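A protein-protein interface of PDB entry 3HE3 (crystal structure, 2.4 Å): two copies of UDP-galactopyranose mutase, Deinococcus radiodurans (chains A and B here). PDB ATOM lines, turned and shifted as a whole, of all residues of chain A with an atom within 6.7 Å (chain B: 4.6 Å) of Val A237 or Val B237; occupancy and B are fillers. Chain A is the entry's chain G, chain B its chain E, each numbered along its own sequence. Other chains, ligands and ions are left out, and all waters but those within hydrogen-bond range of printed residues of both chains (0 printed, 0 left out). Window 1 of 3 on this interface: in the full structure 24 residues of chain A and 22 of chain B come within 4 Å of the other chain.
NZ of Lys B236 sits at hydrogen-bond distance from O of Asn A240 (3.2 Å).
The backbone carbonyl oxygen (O) of Ile B235 lies within hydrogen-bond range of the side-chain amide nitrogen (ND2) of Asn A240 (3.1 Å).
The backbone NH of Leu A239 sits at hydrogen-bond distance from the backbone carbonyl oxygen of Val B237, at 2.9 Å.
The backbone NH of Leu B239 lies within hydrogen-bond range of the backbone carbonyl oxygen of Val A237.
O of Met A238 is in hydrogen-bond range of N of Asp A59 (2.9 Å).
The backbone carbonyl oxygen (O) of Ile B57 is in hydrogen-bond range of the backbone NH (N) of Met B238 (2.8 Å).
N of Lys A236 sits at hydrogen-bond distance from O of Val A55 (3.0 Å).
O of Ile A57 sits at hydrogen-bond distance from N of Met A238.
O of Asp A59 sits at hydrogen-bond distance from N of Thr A241 (2.8 Å).
The backbone NH (N) of Ile A57 lies within hydrogen-bond range of the backbone carbonyl oxygen (O) of Lys A236, at 3.0 Å.
Among the printed residues, pairs that only touch across the chains: Leu A56 with Met B238 (3.5 Å), Lys A236 with Met B238 (3.6 Å), Lys A236 with Leu B239 (3.9 Å), Val A237 with Val B237 (3.6 Å), Val A237 with Met B238 (3.3 Å), Met A238 with Lys B236 (3.8 Å), Met A238 with Val B237 (3.3 Å), Asn A240 with Leu B230 (3.7 Å) and Thr A241 with Lys B236 (3.3 Å).
Val A55 touches none of the printed residues of chain B.
Leu A230 touches none of the printed residues of chain B.
Of the printed residues of chain B, Val A237 touches Val B237 (3.6 Å), Met B238 (3.3 Å) and Leu B239 (2.7 Å).
Printed residues of chain B within 4 Å of Met A238: Lys B236 (3.8 Å) and Val B237 (3.3 Å).
Printed residues of chain B within 4 Å of Leu A239: Val B237.
Of the printed residues of chain A, Val B237 touches Val A237, Met A238 and Leu A239.
The nearest printed residue of chain B that does not touch Val A237 is Ile B57 (6.9 Å).
The nearest printed residue of chain B that does not touch Lys A236 is Val B237 (7.6 Å).
Of the 8 printed residues of chain B, 6 touch a printed residue of chain A.
Hydrophobic or aromatic side chains of chain A within 4 Å of the printed part of chain B: Leu A56 and Met A238.
Lys A236 touches Leu B239, but with the chains exchanged Leu A239 does not touch Lys B236 (4.2 Å).
Val A237 touches its own counterpart, Val B237.
Val A237 touches Met B238, and with the chains exchanged Met A238 touches Val B237.
Val A237 touches Leu B239, and with the chains exchanged Leu A239 touches Val B237.
8 positions are printed for both chains.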
ATOM      1  N   ALA A  37      -0.662  -6.081   7.880  1.00  0.00           N
ATOM      2  CA  ALA A  37       0.431  -6.994   7.559  1.00  0.00           C
ATOM      3  C   ALA A  37       1.787  -6.295   7.470  1.00  0.00           C
ATOM      4  O   ALA A  37       2.637  -6.687   6.671  1.00  0.00           O
ATOM      5  CB  ALA A  37       0.139  -7.745   6.272  1.00  0.00           C
ATOM      6  N   VAL A  55      -3.676 -18.535  12.569  1.00  0.00           N
ATOM      7  CA  VAL A  55      -3.678 -17.085  12.426  1.00  0.00           C
ATOM      8  C   VAL A  55      -4.313 -16.601  11.125  1.00  0.00           C
ATOM      9  O   VAL A  55      -4.094 -17.178  10.059  1.00  0.00           O
ATOM     10  CB  VAL A  55      -2.245 -16.529  12.532  1.00  0.00           C
ATOM     11  CG1 VAL A  55      -2.193 -15.079  12.080  1.00  0.00           C
ATOM     12  CG2 VAL A  55      -1.731 -16.680  13.955  1.00  0.00           C
ATOM     13  N   LEU A  56      -5.110 -15.543  11.225  1.00  0.00           N
ATOM     14  CA  LEU A  56      -5.649 -14.873  10.051  1.00  0.00           C
ATOM     15  C   LEU A  56      -5.159 -13.431  10.042  1.00  0.00           C
ATOM     16  O   LEU A  56      -5.631 -12.603  10.826  1.00  0.00           O
ATOM     17  CB  LEU A  56      -7.181 -14.914  10.055  1.00  0.00           C
ATOM     18  CG  LEU A  56      -7.911 -14.217   8.901  1.00  0.00           C
ATOM     19  CD1 LEU A  56      -7.465 -14.759   7.553  1.00  0.00           C
ATOM     20  CD2 LEU A  56      -9.414 -14.358   9.053  1.00  0.00           C
ATOM     21  N   ILE A  57      -4.193 -13.133   9.178  1.00  0.00           N
ATOM     22  CA  ILE A  57      -3.710 -11.763   9.039  1.00  0.00           C
ATOM     23  C   ILE A  57      -4.382 -11.102   7.844  1.00  0.00           C
ATOM     24  O   ILE A  57      -4.476 -11.682   6.763  1.00  0.00           O
ATOM     25  CB  ILE A  57      -2.163 -11.673   8.947  1.00  0.00           C
ATOM     26  CG1 ILE A  57      -1.714 -10.211   8.996  1.00  0.00           C
ATOM     27  CG2 ILE A  57      -1.642 -12.377   7.699  1.00  0.00           C
ATOM     28  CD1 ILE A  57      -0.249 -10.034   9.311  1.00  0.00           C
ATOM     29  N   VAL A  58      -4.871  -9.887   8.063  1.00  0.00           N
ATOM     30  CA  VAL A  58      -5.692  -9.195   7.082  1.00  0.00           C
ATOM     31  C   VAL A  58      -5.158  -7.769   6.871  1.00  0.00           C
ATOM     32  O   VAL A  58      -4.509  -7.210   7.759  1.00  0.00           O
ATOM     33  CB  VAL A  58      -7.182  -9.195   7.531  1.00  0.00           C
ATOM     34  CG1 VAL A  58      -7.447  -8.099   8.551  1.00  0.00           C
ATOM     35  CG2 VAL A  58      -8.114  -9.061   6.338  1.00  0.00           C
ATOM     36  N   ASP A  59      -5.399  -7.196   5.693  1.00  0.00           N
ATOM     37  CA  ASP A  59      -4.948  -5.833   5.401  1.00  0.00           C
ATOM     38  C   ASP A  59      -5.838  -5.169   4.356  1.00  0.00           C
ATOM     39  O   ASP A  59      -6.221  -5.800   3.372  1.00  0.00           O
ATOM     40  CB  ASP A  59      -3.486  -5.829   4.928  1.00  0.00           C
ATOM     41  CG  ASP A  59      -2.778  -4.508   5.210  1.00  0.00           C
ATOM     42  OD1 ASP A  59      -3.320  -3.437   4.857  1.00  0.00           O
ATOM     43  OD2 ASP A  59      -1.670  -4.543   5.788  1.00  0.00           O
ATOM     44  N   ILE A  64       1.206  -7.129   1.285  1.00  0.00           N
ATOM     45  CA  ILE A  64       1.694  -7.266   2.649  1.00  0.00           C
ATOM     46  C   ILE A  64       2.849  -6.290   2.851  1.00  0.00           C
ATOM     47  O   ILE A  64       3.276  -5.636   1.901  1.00  0.00           O
ATOM     48  CB  ILE A  64       2.180  -8.704   2.916  1.00  0.00           C
ATOM     49  CG1 ILE A  64       3.525  -8.953   2.227  1.00  0.00           C
ATOM     50  CG2 ILE A  64       1.145  -9.712   2.437  1.00  0.00           C
ATOM     51  CD1 ILE A  64       3.971 -10.407   2.251  1.00  0.00           C
ATOM     52  N   LEU A 230       5.673 -14.903   6.535  1.00  0.00           N
ATOM     53  CA  LEU A 230       4.282 -15.349   6.542  1.00  0.00           C
ATOM     54  C   LEU A 230       4.073 -16.655   5.777  1.00  0.00           C
ATOM     55  O   LEU A 230       2.971 -16.921   5.295  1.00  0.00           O
ATOM     56  CB  LEU A 230       3.370 -14.266   5.949  1.00  0.00           C
ATOM     57  CG  LEU A 230       3.465 -12.853   6.530  1.00  0.00           C
ATOM     58  CD1 LEU A 230       2.477 -11.929   5.837  1.00  0.00           C
ATOM     59  CD2 LEU A 230       3.224 -12.862   8.027  1.00  0.00           C
ATOM     60  N   ILE A 235      -0.738 -19.768   8.734  1.00  0.00           N
ATOM     61  CA  ILE A 235      -1.053 -18.378   8.439  1.00  0.00           C
ATOM     62  C   ILE A 235      -1.860 -18.241   7.154  1.00  0.00           C
ATOM     63  O   ILE A 235      -1.411 -18.634   6.077  1.00  0.00           O
ATOM     64  CB  ILE A 235       0.208 -17.494   8.378  1.00  0.00           C
ATOM     65  CG1 ILE A 235       0.939 -17.526   9.721  1.00  0.00           C
ATOM     66  CG2 ILE A 235      -0.162 -16.064   8.027  1.00  0.00           C
ATOM     67  CD1 ILE A 235       2.109 -16.564   9.817  1.00  0.00           C
ATOM     68  N   LYS A 236      -3.068 -17.705   7.295  1.00  0.00           N
ATOM     69  CA  LYS A 236      -3.906 -17.364   6.157  1.00  0.00           C
ATOM     70  C   LYS A 236      -3.782 -15.864   5.944  1.00  0.00           C
ATOM     71  O   LYS A 236      -3.777 -15.097   6.907  1.00  0.00           O
ATOM     72  CB  LYS A 236      -5.361 -17.735   6.436  1.00  0.00           C
ATOM     73  CG  LYS A 236      -5.565 -19.181   6.846  1.00  0.00           C
ATOM     74  CD  LYS A 236      -4.919 -20.128   5.853  1.00  0.00           C
ATOM     75  CE  LYS A 236      -4.801 -21.531   6.420  1.00  0.00           C
ATOM     76  NZ  LYS A 236      -3.796 -22.342   5.676  1.00  0.00           N
ATOM     77  N   VAL A 237      -3.674 -15.441   4.689  1.00  0.00           N
ATOM     78  CA  VAL A 237      -3.493 -14.024   4.395  1.00  0.00           C
ATOM     79  C   VAL A 237      -4.643 -13.451   3.596  1.00  0.00           C
ATOM     80  O   VAL A 237      -4.976 -13.937   2.517  1.00  0.00           O
ATOM     81  CB  VAL A 237      -2.195 -13.752   3.627  1.00  0.00           C
ATOM     82  CG1 VAL A 237      -2.085 -12.273   3.316  1.00  0.00           C
ATOM     83  CG2 VAL A 237      -1.001 -14.220   4.432  1.00  0.00           C
ATOM     84  N   MET A 238      -5.242 -12.398   4.129  1.00  0.00           N
ATOM     85  CA  MET A 238      -6.376 -11.775   3.475  1.00  0.00           C
ATOM     86  C   MET A 238      -6.050 -10.325   3.139  1.00  0.00           C
ATOM     87  O   MET A 238      -5.810  -9.507   4.028  1.00  0.00           O
ATOM     88  CB  MET A 238      -7.602 -11.861   4.373  1.00  0.00           C
ATOM     89  CG  MET A 238      -8.904 -11.978   3.621  1.00  0.00           C
ATOM     90  SD  MET A 238     -10.275 -12.270   4.747  1.00  0.00           S
ATOM     91  CE  MET A 238     -11.657 -11.981   3.643  1.00  0.00           C
ATOM     92  N   LEU A 239      -6.025 -10.019   1.847  1.00  0.00           N
ATOM     93  CA  LEU A 239      -5.669  -8.687   1.384  1.00  0.00           C
ATOM     94  C   LEU A 239      -6.875  -7.982   0.795  1.00  0.00           C
ATOM     95  O   LEU A 239      -7.869  -8.618   0.435  1.00  0.00           O
ATOM     96  CB  LEU A 239      -4.573  -8.774   0.324  1.00  0.00           C
ATOM     97  CG  LEU A 239      -3.328  -9.573   0.695  1.00  0.00           C
ATOM     98  CD1 LEU A 239      -2.581  -9.972  -0.563  1.00  0.00           C
ATOM     99  CD2 LEU A 239      -2.440  -8.772   1.627  1.00  0.00           C
ATOM    100  N   ASN A 240      -6.774  -6.662   0.687  1.00  0.00           N
ATOM    101  CA  ASN A 240      -7.845  -5.867   0.114  1.00  0.00           C
ATOM    102  C   ASN A 240      -9.072  -5.971   1.010  1.00  0.00           C
ATOM    103  O   ASN A 240     -10.207  -5.856   0.545  1.00  0.00           O
ATOM    104  CB  ASN A 240      -8.163  -6.368  -1.298  1.00  0.00           C
ATOM    105  CG  ASN A 240      -8.540  -5.253  -2.245  1.00  0.00           C
ATOM    106  OD1 ASN A 240      -8.100  -4.112  -2.089  1.00  0.00           O
ATOM    107  ND2 ASN A 240      -9.356  -5.578  -3.245  1.00  0.00           N
ATOM    108  N   THR A 241      -8.832  -6.192   2.302  1.00  0.00           N
ATOM    109  CA  THR A 241      -9.910  -6.417   3.255  1.00  0.00           C
ATOM    110  C   THR A 241      -9.757  -5.598   4.532  1.00  0.00           C
ATOM    111  O   THR A 241      -8.759  -5.715   5.243  1.00  0.00           O
ATOM    112  CB  THR A 241     -10.012  -7.907   3.643  1.00  0.00           C
ATOM    113  OG1 THR A 241     -10.170  -8.705   2.463  1.00  0.00           O
ATOM    114  CG2 THR A 241     -11.195  -8.134   4.573  1.00  0.00           C
ATOM    115  N   ILE B  57     -12.270 -14.573  -3.166  1.00  0.00           N
ATOM    116  CA  ILE B  57     -11.454 -15.441  -4.010  1.00  0.00           C
ATOM    117  C   ILE B  57     -10.301 -16.021  -3.201  1.00  0.00           C
ATOM    118  O   ILE B  57      -9.637 -15.313  -2.439  1.00  0.00           O
ATOM    119  CB  ILE B  57     -10.951 -14.723  -5.286  1.00  0.00           C
ATOM    120  CG1 ILE B  57     -10.256 -15.717  -6.220  1.00  0.00           C
ATOM    121  CG2 ILE B  57     -10.041 -13.555  -4.933  1.00  0.00           C
ATOM    122  CD1 ILE B  57     -10.216 -15.268  -7.664  1.00  0.00           C
ATOM    123  N   ILE B  64      -1.522 -14.642  -6.370  1.00  0.00           N
ATOM    124  CA  ILE B  64      -2.588 -14.706  -7.356  1.00  0.00           C
ATOM    125  C   ILE B  64      -2.011 -15.096  -8.720  1.00  0.00           C
ATOM    126  O   ILE B  64      -0.802 -15.269  -8.860  1.00  0.00           O
ATOM    127  CB  ILE B  64      -3.288 -13.347  -7.478  1.00  0.00           C
ATOM    128  CG1 ILE B  64      -2.275 -12.276  -7.890  1.00  0.00           C
ATOM    129  CG2 ILE B  64      -3.940 -12.969  -6.159  1.00  0.00           C
ATOM    130  CD1 ILE B  64      -2.896 -11.039  -8.500  1.00  0.00           C
ATOM    131  N   LEU B 230      -8.348  -7.820 -10.029  1.00  0.00           N
ATOM    132  CA  LEU B 230      -8.880  -8.137  -8.706  1.00  0.00           C
ATOM    133  C   LEU B 230      -8.966  -6.931  -7.766  1.00  0.00           C
ATOM    134  O   LEU B 230      -9.088  -7.101  -6.552  1.00  0.00           O
ATOM    135  CB  LEU B 230      -8.030  -9.229  -8.041  1.00  0.00           C
ATOM    136  CG  LEU B 230      -7.867 -10.565  -8.770  1.00  0.00           C
ATOM    137  CD1 LEU B 230      -7.235 -11.597  -7.852  1.00  0.00           C
ATOM    138  CD2 LEU B 230      -9.205 -11.068  -9.276  1.00  0.00           C
ATOM    139  N   ILE B 235     -14.098  -7.338  -4.062  1.00  0.00           N
ATOM    140  CA  ILE B 235     -13.286  -8.550  -4.068  1.00  0.00           C
ATOM    141  C   ILE B 235     -12.342  -8.635  -2.874  1.00  0.00           C
ATOM    142  O   ILE B 235     -11.585  -7.706  -2.593  1.00  0.00           O
ATOM    143  CB  ILE B 235     -12.472  -8.677  -5.365  1.00  0.00           C
ATOM    144  CG1 ILE B 235     -13.403  -8.949  -6.549  1.00  0.00           C
ATOM    145  CG2 ILE B 235     -11.451  -9.788  -5.240  1.00  0.00           C
ATOM    146  CD1 ILE B 235     -12.730  -8.839  -7.901  1.00  0.00           C
ATOM    147  N   LYS B 236     -12.406  -9.759  -2.169  1.00  0.00           N
ATOM    148  CA  LYS B 236     -11.482 -10.050  -1.087  1.00  0.00           C
ATOM    149  C   LYS B 236     -10.593 -11.206  -1.518  1.00  0.00           C
ATOM    150  O   LYS B 236     -11.085 -12.248  -1.944  1.00  0.00           O
ATOM    151  CB  LYS B 236     -12.242 -10.427   0.183  1.00  0.00           C
ATOM    152  CG  LYS B 236     -13.372  -9.479   0.531  1.00  0.00           C
ATOM    153  CD  LYS B 236     -12.854  -8.072   0.740  1.00  0.00           C
ATOM    154  CE  LYS B 236     -13.950  -7.044   0.538  1.00  0.00           C
ATOM    155  NZ  LYS B 236     -13.386  -5.681   0.347  1.00  0.00           N
ATOM    156  N   VAL B 237      -9.282 -11.019  -1.409  1.00  0.00           N
ATOM    157  CA  VAL B 237      -8.331 -12.046  -1.815  1.00  0.00           C
ATOM    158  C   VAL B 237      -7.789 -12.792  -0.602  1.00  0.00           C
ATOM    159  O   VAL B 237      -7.269 -12.182   0.326  1.00  0.00           O
ATOM    160  CB  VAL B 237      -7.156 -11.436  -2.606  1.00  0.00           C
ATOM    161  CG1 VAL B 237      -6.257 -12.527  -3.136  1.00  0.00           C
ATOM    162  CG2 VAL B 237      -7.682 -10.584  -3.744  1.00  0.00           C
ATOM    163  N   MET B 238      -7.918 -14.113  -0.615  1.00  0.00           N
ATOM    164  CA  MET B 238      -7.387 -14.935   0.466  1.00  0.00           C
ATOM    165  C   MET B 238      -6.317 -15.897  -0.046  1.00  0.00           C
ATOM    166  O   MET B 238      -6.548 -16.663  -0.983  1.00  0.00           O
ATOM    167  CB  MET B 238      -8.506 -15.704   1.164  1.00  0.00           C
ATOM    168  CG  MET B 238      -8.075 -16.361   2.458  1.00  0.00           C
ATOM    169  SD  MET B 238      -9.471 -16.644   3.554  1.00  0.00           S
ATOM    170  CE  MET B 238      -8.624 -17.003   5.090  1.00  0.00           C
ATOM    171  N   LEU B 239      -5.146 -15.853   0.581  1.00  0.00           N
ATOM    172  CA  LEU B 239      -3.988 -16.584   0.087  1.00  0.00           C
ATOM    173  C   LEU B 239      -3.437 -17.580   1.104  1.00  0.00           C
ATOM    174  O   LEU B 239      -3.678 -17.456   2.308  1.00  0.00           O
ATOM    175  CB  LEU B 239      -2.897 -15.603  -0.349  1.00  0.00           C
ATOM    176  CG  LEU B 239      -3.275 -14.736  -1.552  1.00  0.00           C
ATOM    177  CD1 LEU B 239      -2.172 -13.741  -1.877  1.00  0.00           C
ATOM    178  CD2 LEU B 239      -3.591 -15.603  -2.763  1.00  0.00           C
